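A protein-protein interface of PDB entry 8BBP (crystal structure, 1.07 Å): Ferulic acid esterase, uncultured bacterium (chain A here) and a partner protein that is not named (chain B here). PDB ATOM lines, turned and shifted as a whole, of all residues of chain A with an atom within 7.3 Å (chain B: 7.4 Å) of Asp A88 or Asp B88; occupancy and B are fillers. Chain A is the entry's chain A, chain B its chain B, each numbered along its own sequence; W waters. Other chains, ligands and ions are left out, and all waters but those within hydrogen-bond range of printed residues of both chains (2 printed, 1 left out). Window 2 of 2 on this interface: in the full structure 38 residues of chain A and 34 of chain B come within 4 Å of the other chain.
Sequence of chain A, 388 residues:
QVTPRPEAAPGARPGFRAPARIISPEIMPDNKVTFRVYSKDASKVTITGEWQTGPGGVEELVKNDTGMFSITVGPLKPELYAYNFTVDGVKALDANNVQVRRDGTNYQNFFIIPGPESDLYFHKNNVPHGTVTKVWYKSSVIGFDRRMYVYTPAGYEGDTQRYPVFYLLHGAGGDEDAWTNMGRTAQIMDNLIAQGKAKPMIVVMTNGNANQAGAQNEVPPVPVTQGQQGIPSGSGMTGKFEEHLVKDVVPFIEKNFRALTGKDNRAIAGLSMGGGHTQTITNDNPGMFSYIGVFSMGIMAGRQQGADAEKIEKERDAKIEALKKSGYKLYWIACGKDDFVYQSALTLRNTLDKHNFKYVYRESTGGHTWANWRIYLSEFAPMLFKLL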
ATOM      1  N   TYR A  38     -17.361 -16.310 -21.685  1.00  0.00           N
ATOM      2  CA  TYR A  38     -17.965 -16.318 -20.358  1.00  0.00           C
ATOM      3  C   TYR A  38     -18.297 -17.736 -19.913  1.00  0.00           C
ATOM      4  O   TYR A  38     -18.991 -18.469 -20.620  1.00  0.00           O
ATOM      5  CB  TYR A  38     -19.242 -15.481 -20.333  1.00  0.00           C
ATOM      6  CG  TYR A  38     -19.926 -15.572 -18.993  1.00  0.00           C
ATOM      7  CD1 TYR A  38     -19.494 -14.800 -17.929  1.00  0.00           C
ATOM      8  CD2 TYR A  38     -20.972 -16.463 -18.776  1.00  0.00           C
ATOM      9  CE1 TYR A  38     -20.104 -14.891 -16.684  1.00  0.00           C
ATOM     10  CE2 TYR A  38     -21.580 -16.563 -17.545  1.00  0.00           C
ATOM     11  CZ  TYR A  38     -21.145 -15.775 -16.505  1.00  0.00           C
ATOM     12  OH  TYR A  38     -21.748 -15.870 -15.276  1.00  0.00           O
ATOM     13  N   SER A  39     -17.829 -18.105 -18.720  1.00  0.00           N
ATOM     14  CA  SER A  39     -18.341 -19.285 -18.041  1.00  0.00           C
ATOM     15  C   SER A  39     -17.804 -19.366 -16.625  1.00  0.00           C
ATOM     16  O   SER A  39     -16.592 -19.452 -16.416  1.00  0.00           O
ATOM     17  CB  SER A  39     -17.959 -20.581 -18.740  1.00  0.00           C
ATOM     18  OG  SER A  39     -18.328 -21.659 -17.893  1.00  0.00           O
ATOM     19  N   LYS A  40     -18.702 -19.391 -15.651  1.00  0.00           N
ATOM     20  CA  LYS A  40     -18.280 -19.645 -14.286  1.00  0.00           C
ATOM     21  C   LYS A  40     -17.961 -21.110 -14.037  1.00  0.00           C
ATOM     22  O   LYS A  40     -17.299 -21.418 -13.050  1.00  0.00           O
ATOM     23  CB  LYS A  40     -19.364 -19.198 -13.313  1.00  0.00           C
ATOM     24  CG  LYS A  40     -19.458 -17.692 -13.207  1.00  0.00           C
ATOM     25  CD  LYS A  40     -20.486 -17.277 -12.172  1.00  0.00           C
ATOM     26  CE  LYS A  40     -20.521 -15.776 -11.973  1.00  0.00           C
ATOM     27  NZ  LYS A  40     -21.485 -15.392 -10.911  1.00  0.00           N
ATOM     28  N   ASP A  41     -18.420 -22.007 -14.898  1.00  0.00           N
ATOM     29  CA  ASP A  41     -18.210 -23.433 -14.683  1.00  0.00           C
ATOM     30  C   ASP A  41     -16.839 -23.890 -15.164  1.00  0.00           C
ATOM     31  O   ASP A  41     -16.207 -24.733 -14.520  1.00  0.00           O
ATOM     32  CB  ASP A  41     -19.309 -24.220 -15.388  1.00  0.00           C
ATOM     33  CG  ASP A  41     -20.664 -24.018 -14.749  1.00  0.00           C
ATOM     34  OD1 ASP A  41     -20.881 -24.531 -13.637  1.00  0.00           O
ATOM     35  OD2 ASP A  41     -21.505 -23.326 -15.364  1.00  0.00           O
ATOM     36  N   ALA A  42     -16.354 -23.319 -16.264  1.00  0.00           N
ATOM     37  CA  ALA A  42     -15.204 -23.870 -16.954  1.00  0.00           C
ATOM     38  C   ALA A  42     -13.923 -23.653 -16.168  1.00  0.00           C
ATOM     39  O   ALA A  42     -13.755 -22.646 -15.479  1.00  0.00           O
ATOM     40  CB  ALA A  42     -15.078 -23.219 -18.331  1.00  0.00           C
ATOM     41  N   SER A  43     -13.016 -24.627 -16.266  1.00  0.00           N
ATOM     42  CA  SER A  43     -11.701 -24.537 -15.636  1.00  0.00           C
ATOM     43  C   SER A  43     -10.679 -23.859 -16.536  1.00  0.00           C
ATOM     44  O   SER A  43      -9.966 -22.950 -16.102  1.00  0.00           O
ATOM     45  CB  SER A  43     -11.158 -25.925 -15.270  1.00  0.00           C
ATOM     46  OG  SER A  43      -9.777 -25.846 -14.897  1.00  0.00           O
ATOM     47  N   LYS A  44     -10.598 -24.287 -17.789  1.00  0.00           N
ATOM     48  CA  LYS A  44      -9.526 -23.866 -18.671  1.00  0.00           C
ATOM     49  C   LYS A  44     -10.106 -23.585 -20.038  1.00  0.00           C
ATOM     50  O   LYS A  44     -10.763 -24.444 -20.630  1.00  0.00           O
ATOM     51  CB  LYS A  44      -8.462 -24.962 -18.770  1.00  0.00           C
ATOM     52  CG  LYS A  44      -7.289 -24.611 -19.666  1.00  0.00           C
ATOM     53  CD  LYS A  44      -6.191 -25.651 -19.559  1.00  0.00           C
ATOM     54  CE  LYS A  44      -4.982 -25.267 -20.367  1.00  0.00           C
ATOM     55  NZ  LYS A  44      -3.875 -26.231 -20.143  1.00  0.00           N
ATOM     56  N   VAL A  45      -9.850 -22.389 -20.534  1.00  0.00           N
ATOM     57  CA  VAL A  45     -10.228 -22.013 -21.882  1.00  0.00           C
ATOM     58  C   VAL A  45      -8.963 -21.562 -22.582  1.00  0.00           C
ATOM     59  O   VAL A  45      -8.261 -20.666 -22.092  1.00  0.00           O
ATOM     60  CB  VAL A  45     -11.289 -20.902 -21.905  1.00  0.00           C
ATOM     61  CG1 VAL A  45     -11.621 -20.523 -23.349  1.00  0.00           C
ATOM     62  CG2 VAL A  45     -12.533 -21.326 -21.160  1.00  0.00           C
ATOM     63  N   THR A  46      -8.658 -22.192 -23.703  1.00  0.00           N
ATOM     64  CA  THR A  46      -7.540 -21.776 -24.527  1.00  0.00           C
ATOM     65  C   THR A  46      -8.062 -21.296 -25.869  1.00  0.00           C
ATOM     66  O   THR A  46      -9.232 -21.473 -26.212  1.00  0.00           O
ATOM     67  CB  THR A  46      -6.524 -22.907 -24.716  1.00  0.00           C
ATOM     68  OG1 THR A  46      -7.123 -23.960 -25.472  1.00  0.00           O
ATOM     69  CG2 THR A  46      -6.042 -23.441 -23.377  1.00  0.00           C
ATOM     70  N   PHE A  69     -13.425 -15.177 -19.108  1.00  0.00           N
ATOM     71  CA  PHE A  69     -12.098 -15.500 -19.592  1.00  0.00           C
ATOM     72  C   PHE A  69     -11.749 -14.501 -20.685  1.00  0.00           C
ATOM     73  O   PHE A  69     -12.589 -14.168 -21.526  1.00  0.00           O
ATOM     74  CB  PHE A  69     -12.107 -16.892 -20.213  1.00  0.00           C
ATOM     75  CG  PHE A  69     -12.253 -18.030 -19.233  1.00  0.00           C
ATOM     76  CD1 PHE A  69     -13.504 -18.429 -18.781  1.00  0.00           C
ATOM     77  CD2 PHE A  69     -11.139 -18.750 -18.826  1.00  0.00           C
ATOM     78  CE1 PHE A  69     -13.635 -19.503 -17.921  1.00  0.00           C
ATOM     79  CE2 PHE A  69     -11.272 -19.827 -17.976  1.00  0.00           C
ATOM     80  CZ  PHE A  69     -12.523 -20.200 -17.526  1.00  0.00           C
ATOM     81  N   THR A  86     -10.837 -23.775 -27.011  1.00  0.00           N
ATOM     82  CA  THR A  86     -10.984 -25.108 -26.443  1.00  0.00           C
ATOM     83  C   THR A  86     -11.397 -24.909 -24.996  1.00  0.00           C
ATOM     84  O   THR A  86     -10.694 -24.232 -24.235  1.00  0.00           O
ATOM     85  CB  THR A  86      -9.685 -25.914 -26.532  1.00  0.00           C
ATOM     86  OG1 THR A  86      -9.218 -25.927 -27.884  1.00  0.00           O
ATOM     87  CG2 THR A  86      -9.905 -27.339 -26.080  1.00  0.00           C
ATOM     88  N   VAL A  87     -12.543 -25.462 -24.627  1.00  0.00           N
ATOM     89  CA  VAL A  87     -13.109 -25.299 -23.296  1.00  0.00           C
ATOM     90  C   VAL A  87     -13.029 -26.651 -22.629  1.00  0.00           C
ATOM     91  O   VAL A  87     -13.712 -27.594 -23.038  1.00  0.00           O
ATOM     92  CB  VAL A  87     -14.564 -24.825 -23.373  1.00  0.00           C
ATOM     93  CG1 VAL A  87     -15.180 -24.763 -21.978  1.00  0.00           C
ATOM     94  CG2 VAL A  87     -14.660 -23.490 -24.099  1.00  0.00           C
ATOM     95  N   ASP A  88     -12.194 -26.762 -21.604  1.00  0.00           N
ATOM     96  CA  ASP A  88     -12.050 -28.013 -20.877  1.00  0.00           C
ATOM     97  C   ASP A  88     -11.930 -29.192 -21.837  1.00  0.00           C
ATOM     98  O   ASP A  88     -12.558 -30.235 -21.669  1.00  0.00           O
ATOM     99  CB  ASP A  88     -13.174 -28.200 -19.863  1.00  0.00           C
ATOM    100  CG  ASP A  88     -13.156 -27.136 -18.805  1.00  0.00           C
ATOM    101  OD1 ASP A  88     -12.080 -26.571 -18.557  1.00  0.00           O
ATOM    102  OD2 ASP A  88     -14.209 -26.852 -18.211  1.00  0.00           O
ATOM    103  N   GLY A  89     -11.101 -29.010 -22.860  1.00  0.00           N
ATOM    104  CA  GLY A  89     -10.777 -30.061 -23.792  1.00  0.00           C
ATOM    105  C   GLY A  89     -11.690 -30.199 -24.990  1.00  0.00           C
ATOM    106  O   GLY A  89     -11.428 -31.062 -25.829  1.00  0.00           O
ATOM    107  N   VAL A  90     -12.750 -29.401 -25.096  1.00  0.00           N
ATOM    108  CA  VAL A  90     -13.703 -29.492 -26.198  1.00  0.00           C
ATOM    109  C   VAL A  90     -13.585 -28.249 -27.068  1.00  0.00           C
ATOM    110  O   VAL A  90     -13.640 -27.120 -26.572  1.00  0.00           O
ATOM    111  CB  VAL A  90     -15.145 -29.639 -25.684  1.00  0.00           C
ATOM    112  CG1 VAL A  90     -16.106 -29.736 -26.853  1.00  0.00           C
ATOM    113  CG2 VAL A  90     -15.283 -30.849 -24.765  1.00  0.00           C
ATOM    114  N   LYS A  91     -13.454 -28.453 -28.370  1.00  0.00           N
ATOM    115  CA  LYS A  91     -13.467 -27.332 -29.299  1.00  0.00           C
ATOM    116  C   LYS A  91     -14.753 -26.528 -29.165  1.00  0.00           C
ATOM    117  O   LYS A  91     -15.850 -27.087 -29.092  1.00  0.00           O
ATOM    118  CB  LYS A  91     -13.361 -27.868 -30.718  1.00  0.00           C
ATOM    119  CG  LYS A  91     -13.370 -26.779 -31.780  1.00  0.00           C
ATOM    120  CD  LYS A  91     -13.056 -27.332 -33.154  1.00  0.00           C
ATOM    121  CE  LYS A  91     -13.074 -26.241 -34.213  1.00  0.00           C
ATOM    122  NZ  LYS A  91     -12.701 -26.762 -35.549  1.00  0.00           N
ATOM    123  N   TYR B  38     -16.320 -35.968 -26.716  1.00  0.00           N
ATOM    124  CA  TYR B  38     -15.165 -36.533 -26.036  1.00  0.00           C
ATOM    125  C   TYR B  38     -14.367 -35.448 -25.325  1.00  0.00           C
ATOM    126  O   TYR B  38     -13.973 -34.445 -25.932  1.00  0.00           O
ATOM    127  CB  TYR B  38     -14.253 -37.263 -27.020  1.00  0.00           C
ATOM    128  CG  TYR B  38     -13.014 -37.778 -26.346  1.00  0.00           C
ATOM    129  CD1 TYR B  38     -13.055 -38.930 -25.576  1.00  0.00           C
ATOM    130  CD2 TYR B  38     -11.810 -37.096 -26.443  1.00  0.00           C
ATOM    131  CE1 TYR B  38     -11.930 -39.397 -24.937  1.00  0.00           C
ATOM    132  CE2 TYR B  38     -10.680 -37.556 -25.805  1.00  0.00           C
ATOM    133  CZ  TYR B  38     -10.748 -38.706 -25.054  1.00  0.00           C
ATOM    134  OH  TYR B  38      -9.625 -39.172 -24.418  1.00  0.00           O
ATOM    135  N   SER B  39     -14.142 -35.655 -24.034  1.00  0.00           N
ATOM    136  CA  SER B  39     -13.124 -34.914 -23.304  1.00  0.00           C
ATOM    137  C   SER B  39     -12.957 -35.479 -21.909  1.00  0.00           C
ATOM    138  O   SER B  39     -13.896 -35.471 -21.108  1.00  0.00           O
ATOM    139  CB  SER B  39     -13.466 -33.441 -23.145  1.00  0.00           C
ATOM    140  OG  SER B  39     -12.498 -32.857 -22.280  1.00  0.00           O
ATOM    141  N   LYS B  40     -11.752 -35.936 -21.599  1.00  0.00           N
ATOM    142  CA  LYS B  40     -11.462 -36.365 -20.241  1.00  0.00           C
ATOM    143  C   LYS B  40     -11.492 -35.204 -19.258  1.00  0.00           C
ATOM    144  O   LYS B  40     -11.661 -35.433 -18.059  1.00  0.00           O
ATOM    145  CB  LYS B  40     -10.104 -37.066 -20.205  1.00  0.00           C
ATOM    146  CG  LYS B  40     -10.110 -38.390 -20.953  1.00  0.00           C
ATOM    147  CD  LYS B  40      -8.824 -39.183 -20.793  1.00  0.00           C
ATOM    148  CE  LYS B  40      -8.986 -40.588 -21.393  1.00  0.00           C
ATOM    149  NZ  LYS B  40      -7.731 -41.373 -21.377  1.00  0.00           N
ATOM    150  N   ASP B  41     -11.373 -33.967 -19.738  1.00  0.00           N
ATOM    151  CA  ASP B  41     -11.225 -32.814 -18.865  1.00  0.00           C
ATOM    152  C   ASP B  41     -12.510 -32.039 -18.642  1.00  0.00           C
ATOM    153  O   ASP B  41     -12.509 -31.095 -17.851  1.00  0.00           O
ATOM    154  CB  ASP B  41     -10.163 -31.871 -19.435  1.00  0.00           C
ATOM    155  CG  ASP B  41      -8.795 -32.500 -19.431  1.00  0.00           C
ATOM    156  OD1 ASP B  41      -8.469 -33.175 -18.439  1.00  0.00           O
ATOM    157  OD2 ASP B  41      -8.066 -32.356 -20.427  1.00  0.00           O
ATOM    158  N   ALA B  42     -13.589 -32.382 -19.322  1.00  0.00           N
ATOM    159  CA  ALA B  42     -14.835 -31.661 -19.123  1.00  0.00           C
ATOM    160  C   ALA B  42     -15.629 -32.298 -17.995  1.00  0.00           C
ATOM    161  O   ALA B  42     -15.524 -33.501 -17.738  1.00  0.00           O
ATOM    162  CB  ALA B  42     -15.672 -31.658 -20.399  1.00  0.00           C
ATOM    163  N   SER B  43     -16.418 -31.473 -17.310  1.00  0.00           N
ATOM    164  CA  SER B  43     -17.229 -31.935 -16.191  1.00  0.00           C
ATOM    165  C   SER B  43     -18.647 -32.268 -16.613  1.00  0.00           C
ATOM    166  O   SER B  43     -19.179 -33.306 -16.215  1.00  0.00           O
ATOM    167  CB  SER B  43     -17.280 -30.876 -15.086  1.00  0.00           C
ATOM    168  OG  SER B  43     -17.968 -31.379 -13.957  1.00  0.00           O
ATOM    169  N   LYS B  44     -19.273 -31.391 -17.395  1.00  0.00           N
ATOM    170  CA  LYS B  44     -20.686 -31.493 -17.717  1.00  0.00           C
ATOM    171  C   LYS B  44     -20.898 -31.091 -19.165  1.00  0.00           C
ATOM    172  O   LYS B  44     -20.398 -30.053 -19.604  1.00  0.00           O
ATOM    173  CB  LYS B  44     -21.510 -30.557 -16.835  1.00  0.00           C
ATOM    174  CG  LYS B  44     -22.998 -30.800 -16.966  1.00  0.00           C
ATOM    175  CD  LYS B  44     -23.840 -29.774 -16.229  1.00  0.00           C
ATOM    176  CE  LYS B  44     -25.279 -30.256 -16.134  1.00  0.00           C
ATOM    177  NZ  LYS B  44     -26.227 -29.175 -15.749  1.00  0.00           N
ATOM    178  N   VAL B  45     -21.661 -31.892 -19.894  1.00  0.00           N
ATOM    179  CA  VAL B  45     -22.057 -31.556 -21.252  1.00  0.00           C
ATOM    180  C   VAL B  45     -23.556 -31.751 -21.334  1.00  0.00           C
ATOM    181  O   VAL B  45     -24.068 -32.816 -20.971  1.00  0.00           O
ATOM    182  CB  VAL B  45     -21.342 -32.427 -22.298  1.00  0.00           C
ATOM    183  CG1 VAL B  45     -21.769 -32.027 -23.697  1.00  0.00           C
ATOM    184  CG2 VAL B  45     -19.833 -32.326 -22.143  1.00  0.00           C
ATOM    185  N   THR B  46     -24.256 -30.729 -21.798  1.00  0.00           N
ATOM    186  CA  THR B  46     -25.677 -30.850 -22.065  1.00  0.00           C
ATOM    187  C   THR B  46     -25.928 -30.651 -23.553  1.00  0.00           C
ATOM    188  O   THR B  46     -25.047 -30.233 -24.309  1.00  0.00           O
ATOM    189  CB  THR B  46     -26.493 -29.836 -21.258  1.00  0.00           C
ATOM    190  OG1 THR B  46     -26.180 -28.524 -21.715  1.00  0.00           O
ATOM    191  CG2 THR B  46     -26.186 -29.944 -19.775  1.00  0.00           C
ATOM    192  N   PHE B  69     -18.743 -38.490 -23.342  1.00  0.00           N
ATOM    193  CA  PHE B  69     -20.088 -38.107 -22.947  1.00  0.00           C
ATOM    194  C   PHE B  69     -21.044 -38.554 -24.039  1.00  0.00           C
ATOM    195  O   PHE B  69     -20.749 -38.403 -25.228  1.00  0.00           O
ATOM    196  CB  PHE B  69     -20.201 -36.585 -22.836  1.00  0.00           C
ATOM    197  CG  PHE B  69     -19.405 -35.975 -21.715  1.00  0.00           C
ATOM    198  CD1 PHE B  69     -18.039 -35.749 -21.825  1.00  0.00           C
ATOM    199  CD2 PHE B  69     -20.049 -35.583 -20.565  1.00  0.00           C
ATOM    200  CE1 PHE B  69     -17.339 -35.167 -20.783  1.00  0.00           C
ATOM    201  CE2 PHE B  69     -19.359 -34.999 -19.526  1.00  0.00           C
ATOM    202  CZ  PHE B  69     -18.005 -34.789 -19.637  1.00  0.00           C
ATOM    203  N   THR B  86     -23.660 -27.679 -24.711  1.00  0.00           N
ATOM    204  CA  THR B  86     -23.080 -26.722 -23.782  1.00  0.00           C
ATOM    205  C   THR B  86     -22.074 -27.510 -22.965  1.00  0.00           C
ATOM    206  O   THR B  86     -22.442 -28.486 -22.307  1.00  0.00           O
ATOM    207  CB  THR B  86     -24.129 -26.078 -22.876  1.00  0.00           C
ATOM    208  OG1 THR B  86     -25.158 -25.504 -23.682  1.00  0.00           O
ATOM    209  CG2 THR B  86     -23.504 -24.976 -22.033  1.00  0.00           C
ATOM    210  N   VAL B  87     -20.812 -27.101 -23.020  1.00  0.00           N
ATOM    211  CA  VAL B  87     -19.716 -27.782 -22.341  1.00  0.00           C
ATOM    212  C   VAL B  87     -19.258 -26.866 -21.225  1.00  0.00           C
ATOM    213  O   VAL B  87     -18.766 -25.765 -21.486  1.00  0.00           O
ATOM    214  CB  VAL B  87     -18.549 -28.074 -23.293  1.00  0.00           C
ATOM    215  CG1 VAL B  87     -17.376 -28.712 -22.523  1.00  0.00           C
ATOM    216  CG2 VAL B  87     -19.008 -28.941 -24.446  1.00  0.00           C
ATOM    217  N   ASP B  88     -19.431 -27.296 -19.979  1.00  0.00           N
ATOM    218  CA  ASP B  88     -18.979 -26.519 -18.832  1.00  0.00           C
ATOM    219  C   ASP B  88     -19.361 -25.051 -18.991  1.00  0.00           C
ATOM    220  O   ASP B  88     -18.568 -24.136 -18.772  1.00  0.00           O
ATOM    221  CB  ASP B  88     -17.485 -26.710 -18.598  1.00  0.00           C
ATOM    222  CG  ASP B  88     -17.145 -28.136 -18.243  1.00  0.00           C
ATOM    223  OD1 ASP B  88     -18.075 -28.876 -17.861  1.00  0.00           O
ATOM    224  OD2 ASP B  88     -15.955 -28.529 -18.319  1.00  0.00           O
ATOM    225  N   GLY B  89     -20.618 -24.842 -19.370  1.00  0.00           N
ATOM    226  CA  GLY B  89     -21.210 -23.530 -19.458  1.00  0.00           C
ATOM    227  C   GLY B  89     -20.978 -22.775 -20.746  1.00  0.00           C
ATOM    228  O   GLY B  89     -21.443 -21.639 -20.847  1.00  0.00           O
ATOM    229  N   VAL B  90     -20.296 -23.352 -21.735  1.00  0.00           N
ATOM    230  CA  VAL B  90     -19.989 -22.675 -22.992  1.00  0.00           C
ATOM    231  C   VAL B  90     -20.679 -23.413 -24.136  1.00  0.00           C
ATOM    232  O   VAL B  90     -20.535 -24.630 -24.281  1.00  0.00           O
ATOM    233  CB  VAL B  90     -18.475 -22.602 -23.239  1.00  0.00           C
ATOM    234  CG1 VAL B  90     -18.190 -21.858 -24.535  1.00  0.00           C
ATOM    235  CG2 VAL B  90     -17.783 -21.909 -22.076  1.00  0.00           C
ATOM    236  N   LYS B  91     -21.385 -22.672 -24.979  1.00  0.00           N
ATOM    237  CA  LYS B  91     -21.964 -23.268 -26.175  1.00  0.00           C
ATOM    238  C   LYS B  91     -20.878 -23.916 -27.017  1.00  0.00           C
ATOM    239  O   LYS B  91     -19.815 -23.339 -27.248  1.00  0.00           O
ATOM    240  CB  LYS B  91     -22.656 -22.189 -26.998  1.00  0.00           C
ATOM    241  CG  LYS B  91     -23.239 -22.721 -28.303  1.00  0.00           C
ATOM    242  CD  LYS B  91     -24.056 -21.683 -29.036  1.00  0.00           C
ATOM    243  CE  LYS B  91     -24.624 -22.242 -30.314  1.00  0.00           C
ATOM    244  NZ  LYS B  91     -25.497 -21.248 -30.998  1.00  0.00           N
HETATM  245  O   HOH W   1     -12.641 -33.170 -27.774  1.00  0.00           O
HETATM  246  O   HOH W   2     -21.153 -18.849 -22.160  1.00  0.00           O
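OG of Ser A39 is in hydrogen-bond range of O of Asp B88.
The backbone carbonyl oxygen (O) of Asp B88 lies within hydrogen-bond range of the backbone NH (N) of Ala A42 (3.4 Å).
The backbone carbonyl oxygen of Asp A88 is in hydrogen-bond range of the side-chain hydroxyl of Ser B39 (2.7 Å).
N of Ala B42 lies within hydrogen-bond range of O of Asp A88, 3.3 Å away.
The side-chain carboxylate of Asp A88 lies close to the side-chain carboxylate of Asp B88 (2.4 Å).
The backbone NH (N) of Asp A41 sits at hydrogen-bond distance from the side-chain hydroxyl (OG) of Ser A39, 3.0 Å away.
The backbone NH (N) of Lys A44 sits at hydrogen-bond distance from the side-chain carboxylate (OD1) of Asp A88 (2.8 Å).
N of Asp B41 is in hydrogen-bond range of OG of Ser B39 (3.0 Å).
The backbone NH (N) of Ala B42 lies within hydrogen-bond range of the side-chain hydroxyl (OG) of Ser B39, 3.2 Å away.
N of Ser B43 sits at hydrogen-bond distance from OD1 of Asp B88 (3.1 Å).
N of Lys B44 is in hydrogen-bond range of OD1 of Asp B88, 2.8 Å away.
Tyr A38 touches Val B90.
OG of Ser A39 touches CA of Gly B89, at 3.8 Å.
Ser A39 touches Val B90.
O of Asp B88 touches CB of Asp A41, at 3.5 Å.
Val A87 touches Val B87.
Val A87 touches Val B90 (CG1 to CG2, 3.9 Å).
Asp B41 touches Asp A88.
CA of Gly A89 touches OG of Ser B39, 3.6 Å away.
Val A90 touches Ser B39 (CG2 to CB, 3.6 Å).
CG1 of Val B87 touches CG2 of Val A90 (3.7 Å).
Asp A88 touches just these residues of chain B: Ser B39 (2.7 Å), Asp B41 (3.5 Å), Ala B42 (3.3 Å) and Asp B88 (2.4 Å).
Printed residues of chain A within 4 Å of Asp B88: Ser A39 (2.6 Å), Asp A41 (3.5 Å), Ala A42 (3.4 Å) and Asp A88 (2.4 Å).
Of the printed residues of chain B, Ser A39 touches Asp B88 (2.6 Å), Gly B89 (3.8 Å) and Val B90 (3.6 Å).
Printed residues of chain A within 4 Å of Val B90: Tyr A38, Ser A39 and Val A87.
Of the printed residues of chain A, Ala B42 touches Asp A88 (3.3 Å).
The nearest printed residue of chain B that does not touch Asp A88 is Val B87 (5.0 Å).
Printed residues of chain B that touch a printed residue of chain A: Ser B39, Asp B41, Ala B42, Val B87, Asp B88, Gly B89 and Val B90.
Hydrophobic or aromatic side chains of chain B that line the printed part of chain A: Ala B42, Val B87 and Val B90.
Of the 16 printed residues of chain A, 8 touch a printed residue of chain B.
Printed residues of chain A that touch a printed residue of chain B: Tyr A38, Ser A39, Asp A41, Ala A42, Val A87, Asp A88, Gly A89 and Val A90.
Hydrophobic or aromatic side chains of chain A within 4 Å of the printed part of chain B: Ala A42, Val A87 and Val A90.
Among the printed residues, no Asp or Glu carboxylate lies within 4 Å of a Lys or Arg side-chain nitrogen of the other chain.
Water W1 bridges the backbone carbonyl oxygen of Tyr B38 (2.6 Å) and the backbone carbonyl oxygen of Gly A89 (3.1 Å).
Water W2 lies within hydrogen-bond range of O of Tyr A38 (2.7 Å) and O of Gly B89 (3.1 Å).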
